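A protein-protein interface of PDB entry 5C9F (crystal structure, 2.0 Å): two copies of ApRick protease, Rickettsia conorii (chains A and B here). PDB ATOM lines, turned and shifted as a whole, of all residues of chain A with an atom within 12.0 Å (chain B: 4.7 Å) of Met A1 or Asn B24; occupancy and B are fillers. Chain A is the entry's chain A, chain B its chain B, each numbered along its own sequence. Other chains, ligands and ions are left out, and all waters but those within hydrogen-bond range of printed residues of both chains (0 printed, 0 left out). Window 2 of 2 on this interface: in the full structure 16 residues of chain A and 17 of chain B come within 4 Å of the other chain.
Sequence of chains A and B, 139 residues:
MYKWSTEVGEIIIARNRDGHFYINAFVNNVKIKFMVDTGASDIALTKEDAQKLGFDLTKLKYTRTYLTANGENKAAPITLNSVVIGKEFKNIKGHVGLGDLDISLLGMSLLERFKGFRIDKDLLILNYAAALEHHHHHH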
ATOM      1  N   MET A   1      24.781 -24.002 -18.233  1.00  0.00           N
ATOM      2  CA  MET A   1      24.221 -24.816 -19.331  1.00  0.00           C
ATOM      3  C   MET A   1      25.074 -26.021 -19.644  1.00  0.00           C
ATOM      4  O   MET A   1      26.290 -25.920 -19.751  1.00  0.00           O
ATOM      5  CB  MET A   1      24.170 -24.035 -20.672  1.00  0.00           C
ATOM      6  CG  MET A   1      22.770 -23.617 -21.125  1.00  0.00           C
ATOM      7  SD  MET A   1      22.504 -21.960 -21.819  1.00  0.00           S
ATOM      8  CE  MET A   1      23.039 -22.401 -23.446  1.00  0.00           C
ATOM      9  N   TYR A   2      24.405 -27.121 -19.956  1.00  0.00           N
ATOM     10  CA  TYR A   2      25.029 -28.198 -20.640  1.00  0.00           C
ATOM     11  C   TYR A   2      24.491 -28.263 -22.061  1.00  0.00           C
ATOM     12  O   TYR A   2      23.301 -28.172 -22.314  1.00  0.00           O
ATOM     13  CB  TYR A   2      24.773 -29.506 -19.894  1.00  0.00           C
ATOM     14  CG  TYR A   2      25.441 -30.688 -20.563  1.00  0.00           C
ATOM     15  CD1 TYR A   2      26.828 -30.835 -20.553  1.00  0.00           C
ATOM     16  CD2 TYR A   2      24.690 -31.668 -21.214  1.00  0.00           C
ATOM     17  CE1 TYR A   2      27.444 -31.935 -21.149  1.00  0.00           C
ATOM     18  CE2 TYR A   2      25.296 -32.769 -21.796  1.00  0.00           C
ATOM     19  CZ  TYR A   2      26.671 -32.907 -21.761  1.00  0.00           C
ATOM     20  OH  TYR A   2      27.257 -34.007 -22.346  1.00  0.00           O
ATOM     21  N   LYS A   3      25.400 -28.496 -22.990  1.00  0.00           N
ATOM     22  CA  LYS A   3      25.058 -28.708 -24.386  1.00  0.00           C
ATOM     23  C   LYS A   3      25.849 -29.883 -24.930  1.00  0.00           C
ATOM     24  O   LYS A   3      27.055 -29.998 -24.718  1.00  0.00           O
ATOM     25  CB  LYS A   3      25.370 -27.461 -25.195  1.00  0.00           C
ATOM     26  CG  LYS A   3      24.910 -27.512 -26.638  1.00  0.00           C
ATOM     27  CD  LYS A   3      25.137 -26.144 -27.279  1.00  0.00           C
ATOM     28  CE  LYS A   3      24.596 -26.091 -28.701  1.00  0.00           C
ATOM     29  NZ  LYS A   3      25.367 -26.939 -29.663  1.00  0.00           N
ATOM     30  N   TRP A   4      25.166 -30.737 -25.671  1.00  0.00           N
ATOM     31  CA  TRP A   4      25.794 -31.882 -26.254  1.00  0.00           C
ATOM     32  C   TRP A   4      25.105 -32.131 -27.586  1.00  0.00           C
ATOM     33  O   TRP A   4      23.912 -31.926 -27.715  1.00  0.00           O
ATOM     34  CB  TRP A   4      25.692 -33.112 -25.337  1.00  0.00           C
ATOM     35  CG  TRP A   4      26.619 -34.192 -25.823  1.00  0.00           C
ATOM     36  CD1 TRP A   4      27.994 -34.280 -25.636  1.00  0.00           C
ATOM     37  CD2 TRP A   4      26.275 -35.258 -26.662  1.00  0.00           C
ATOM     38  NE1 TRP A   4      28.491 -35.364 -26.290  1.00  0.00           N
ATOM     39  CE2 TRP A   4      27.464 -35.978 -26.944  1.00  0.00           C
ATOM     40  CE3 TRP A   4      25.060 -35.694 -27.207  1.00  0.00           C
ATOM     41  CZ2 TRP A   4      27.470 -37.129 -27.711  1.00  0.00           C
ATOM     42  CZ3 TRP A   4      25.064 -36.855 -27.972  1.00  0.00           C
ATOM     43  CH2 TRP A   4      26.260 -37.545 -28.223  1.00  0.00           C
ATOM     44  N   SER A   5      25.860 -32.469 -28.610  1.00  0.00           N
ATOM     45  CA  SER A   5      25.229 -32.847 -29.879  1.00  0.00           C
ATOM     46  C   SER A   5      25.992 -33.923 -30.627  1.00  0.00           C
ATOM     47  O   SER A   5      27.209 -34.035 -30.506  1.00  0.00           O
ATOM     48  CB  SER A   5      24.974 -31.652 -30.792  1.00  0.00           C
ATOM     49  OG  SER A   5      26.183 -31.081 -31.300  1.00  0.00           O
ATOM     50  N   ILE B  11      20.092 -29.427 -24.783  1.00  0.00           N
ATOM     51  CA  ILE B  11      20.527 -28.407 -23.874  1.00  0.00           C
ATOM     52  C   ILE B  11      19.822 -28.587 -22.518  1.00  0.00           C
ATOM     53  O   ILE B  11      18.617 -28.825 -22.462  1.00  0.00           O
ATOM     54  CB  ILE B  11      20.187 -27.022 -24.417  1.00  0.00           C
ATOM     55  CG1 ILE B  11      20.958 -26.803 -25.735  1.00  0.00           C
ATOM     56  CG2 ILE B  11      20.606 -25.976 -23.406  1.00  0.00           C
ATOM     57  CD1 ILE B  11      20.345 -25.771 -26.610  1.00  0.00           C
ATOM     58  N   ILE B  12      20.605 -28.625 -21.454  1.00  0.00           N
ATOM     59  CA  ILE B  12      20.084 -28.888 -20.114  1.00  0.00           C
ATOM     60  C   ILE B  12      20.470 -27.707 -19.292  1.00  0.00           C
ATOM     61  O   ILE B  12      21.654 -27.349 -19.250  1.00  0.00           O
ATOM     62  CB  ILE B  12      20.707 -30.134 -19.460  1.00  0.00           C
ATOM     63  CG1 ILE B  12      20.395 -31.382 -20.290  1.00  0.00           C
ATOM     64  CG2 ILE B  12      20.164 -30.323 -18.050  1.00  0.00           C
ATOM     65  CD1 ILE B  12      21.251 -32.572 -19.910  1.00  0.00           C
ATOM     66  N   ILE B  13      19.481 -27.127 -18.617  1.00  0.00           N
ATOM     67  CA  ILE B  13      19.723 -25.955 -17.797  1.00  0.00           C
ATOM     68  C   ILE B  13      19.193 -26.184 -16.411  1.00  0.00           C
ATOM     69  O   ILE B  13      18.050 -26.605 -16.241  1.00  0.00           O
ATOM     70  CB  ILE B  13      19.076 -24.738 -18.437  1.00  0.00           C
ATOM     71  CG1 ILE B  13      19.886 -24.392 -19.693  1.00  0.00           C
ATOM     72  CG2 ILE B  13      19.109 -23.523 -17.508  1.00  0.00           C
ATOM     73  CD1 ILE B  13      19.096 -23.754 -20.772  1.00  0.00           C
ATOM     74  N   TYR B  22      17.553 -19.499 -16.830  1.00  0.00           N
ATOM     75  CA  TYR B  22      18.179 -18.615 -17.796  1.00  0.00           C
ATOM     76  C   TYR B  22      18.836 -19.402 -18.946  1.00  0.00           C
ATOM     77  O   TYR B  22      19.396 -20.479 -18.735  1.00  0.00           O
ATOM     78  CB  TYR B  22      19.205 -17.739 -17.097  1.00  0.00           C
ATOM     79  CG  TYR B  22      18.584 -16.908 -15.988  1.00  0.00           C
ATOM     80  CD1 TYR B  22      18.029 -15.664 -16.258  1.00  0.00           C
ATOM     81  CD2 TYR B  22      18.534 -17.384 -14.689  1.00  0.00           C
ATOM     82  CE1 TYR B  22      17.455 -14.908 -15.251  1.00  0.00           C
ATOM     83  CE2 TYR B  22      17.950 -16.643 -13.662  1.00  0.00           C
ATOM     84  CZ  TYR B  22      17.429 -15.402 -13.955  1.00  0.00           C
ATOM     85  OH  TYR B  22      16.855 -14.690 -12.975  1.00  0.00           O
ATOM     86  N   ILE B  23      18.754 -18.859 -20.158  1.00  0.00           N
ATOM     87  CA  ILE B  23      19.364 -19.467 -21.367  1.00  0.00           C
ATOM     88  C   ILE B  23      20.096 -18.429 -22.193  1.00  0.00           C
ATOM     89  O   ILE B  23      19.565 -17.368 -22.434  1.00  0.00           O
ATOM     90  CB  ILE B  23      18.378 -20.048 -22.371  1.00  0.00           C
ATOM     91  CG1 ILE B  23      17.377 -20.973 -21.728  1.00  0.00           C
ATOM     92  CG2 ILE B  23      19.153 -20.866 -23.418  1.00  0.00           C
ATOM     93  CD1 ILE B  23      16.341 -21.425 -22.741  1.00  0.00           C
ATOM     94  N   ASN B  24      21.308 -18.749 -22.581  1.00  0.00           N
ATOM     95  CA  ASN B  24      22.071 -17.950 -23.494  1.00  0.00           C
ATOM     96  C   ASN B  24      21.713 -18.373 -24.926  1.00  0.00           C
ATOM     97  O   ASN B  24      21.770 -19.549 -25.261  1.00  0.00           O
ATOM     98  CB  ASN B  24      23.544 -18.159 -23.213  1.00  0.00           C
ATOM     99  CG  ASN B  24      23.974 -17.510 -21.905  1.00  0.00           C
ATOM    100  OD1 ASN B  24      23.599 -16.372 -21.592  1.00  0.00           O
ATOM    101  ND2 ASN B  24      24.703 -18.246 -21.121  1.00  0.00           N
ATOM    102  N   ALA B  25      21.340 -17.417 -25.756  1.00  0.00           N
ATOM    103  CA  ALA B  25      21.096 -17.652 -27.169  1.00  0.00           C
ATOM    104  C   ALA B  25      21.948 -16.710 -27.997  1.00  0.00           C
ATOM    105  O   ALA B  25      22.368 -15.656 -27.530  1.00  0.00           O
ATOM    106  CB  ALA B  25      19.642 -17.393 -27.472  1.00  0.00           C
ATOM    107  N   PHE B  26      22.248 -17.108 -29.218  1.00  0.00           N
ATOM    108  CA  PHE B  26      22.927 -16.222 -30.155  1.00  0.00           C
ATOM    109  C   PHE B  26      21.889 -15.676 -31.109  1.00  0.00           C
ATOM    110  O   PHE B  26      21.314 -16.409 -31.894  1.00  0.00           O
ATOM    111  CB  PHE B  26      24.046 -16.935 -30.936  1.00  0.00           C
ATOM    112  CG  PHE B  26      25.195 -17.306 -30.092  1.00  0.00           C
ATOM    113  CD1 PHE B  26      26.253 -16.438 -29.966  1.00  0.00           C
ATOM    114  CD2 PHE B  26      25.221 -18.512 -29.410  1.00  0.00           C
ATOM    115  CE1 PHE B  26      27.335 -16.771 -29.176  1.00  0.00           C
ATOM    116  CE2 PHE B  26      26.305 -18.849 -28.606  1.00  0.00           C
ATOM    117  CZ  PHE B  26      27.360 -17.965 -28.501  1.00  0.00           C
ATOM    118  N   LYS B  31      25.529 -13.002 -28.434  1.00  0.00           N
ATOM    119  CA  LYS B  31      25.115 -13.788 -27.290  1.00  0.00           C
ATOM    120  C   LYS B  31      24.227 -12.911 -26.424  1.00  0.00           C
ATOM    121  O   LYS B  31      24.569 -11.783 -26.095  1.00  0.00           O
ATOM    122  CB  LYS B  31      26.303 -14.237 -26.477  1.00  0.00           C
ATOM    123  CG  LYS B  31      25.932 -15.141 -25.314  1.00  0.00           C
ATOM    124  CD  LYS B  31      27.112 -15.182 -24.362  1.00  0.00           C
ATOM    125  CE  LYS B  31      26.972 -16.220 -23.282  1.00  0.00           C
ATOM    126  NZ  LYS B  31      28.202 -16.188 -22.442  1.00  0.00           N
ATOM    127  N   ILE B  32      23.030 -13.398 -26.155  1.00  0.00           N
ATOM    128  CA  ILE B  32      22.033 -12.647 -25.365  1.00  0.00           C
ATOM    129  C   ILE B  32      21.608 -13.620 -24.272  1.00  0.00           C
ATOM    130  O   ILE B  32      21.359 -14.804 -24.544  1.00  0.00           O
ATOM    131  CB  ILE B  32      20.774 -12.257 -26.192  1.00  0.00           C
ATOM    132  CG1 ILE B  32      21.074 -11.344 -27.397  1.00  0.00           C
ATOM    133  CG2 ILE B  32      19.714 -11.588 -25.297  1.00  0.00           C
ATOM    134  CD1 ILE B  32      21.530  -9.971 -27.040  1.00  0.00           C
ATOM    135  N   LYS B  33      21.434 -13.113 -23.066  1.00  0.00           N
ATOM    136  CA  LYS B  33      20.946 -13.913 -21.949  1.00  0.00           C
ATOM    137  C   LYS B  33      19.460 -13.692 -21.745  1.00  0.00           C
ATOM    138  O   LYS B  33      18.982 -12.561 -21.626  1.00  0.00           O
ATOM    139  CB  LYS B  33      21.663 -13.536 -20.667  1.00  0.00           C
ATOM    140  CG  LYS B  33      21.369 -14.508 -19.532  1.00  0.00           C
ATOM    141  CD  LYS B  33      21.991 -14.015 -18.243  1.00  0.00           C
ATOM    142  CE  LYS B  33      22.156 -15.142 -17.260  1.00  0.00           C
ATOM    143  NZ  LYS B  33      22.611 -14.624 -15.947  1.00  0.00           N
ATOM    144  N   ILE B  85      19.806 -21.469 -30.552  1.00  0.00           N
ATOM    145  CA  ILE B  85      19.883 -22.139 -29.246  1.00  0.00           C
ATOM    146  C   ILE B  85      20.010 -23.616 -29.580  1.00  0.00           C
ATOM    147  O   ILE B  85      18.995 -24.311 -29.712  1.00  0.00           O
ATOM    148  CB  ILE B  85      18.603 -21.941 -28.411  1.00  0.00           C
ATOM    149  CG1 ILE B  85      18.371 -20.449 -28.112  1.00  0.00           C
ATOM    150  CG2 ILE B  85      18.713 -22.662 -27.055  1.00  0.00           C
ATOM    151  CD1 ILE B  85      16.992 -20.148 -27.566  1.00  0.00           C
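SD of Met A1 is in hydrogen-bond range of N of Asn B24, at 3.5 Å.
The backbone NH (N) of Tyr A2 sits at hydrogen-bond distance from the backbone carbonyl oxygen (O) of Ile B12 (2.8 Å).
CG of Met A1 touches CG2 of Ile B11, at 3.9 Å.
Ile B12 touches Met A1.
Met A1 touches Ile B13 (CG to CG1, 3.3 Å).
SD of Met A1 touches CG2 of Ile B23 (3.9 Å).
Ile B11 touches Tyr A2 (CA to O, 3.2 Å).
Of the printed residues of chain B, Met A1 touches Ile B11 (3.9 Å), Ile B12 (3.6 Å), Ile B13 (3.3 Å), Ile B23 (3.9 Å) and Asn B24 (3.5 Å).
Of the printed residues of chain B, Tyr A2 touches Ile B11 (3.2 Å) and Ile B12 (2.8 Å).
Ile B11 touches just these residues of chain A: Met A1 and Tyr A2.
Of chain A, only Met A1 (3.6 Å) and Tyr A2 (2.8 Å) come within 4 Å of Ile B12.
Ile B13 touches just one residue of chain A: Met A1.
Of chain A, only Met A1 (3.9 Å) comes within 4 Å of Ile B23.
No residue of chain A comes within 4 Å of Ala B25.
No residue of chain A comes within 4 Å of Lys B31.
No residue of chain A comes within 4 Å of Lys B33.
The nearest residue of chain B that does not touch Met A1 is Tyr B22 (4.6 Å).
Hydrophobic or aromatic side chains of chain A within 4 Å of the printed part of chain B: Met A1 and Tyr A2.
Hydrophobic or aromatic side chains of chain B that line the printed part of chain A: Ile B11, Ile B12, Ile B13 and Ile B23.
Among the printed residues, no Asp or Glu carboxylate lies within 4 Å of a Lys or Arg side-chain nitrogen of the other chain.
No position is printed for both chains.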
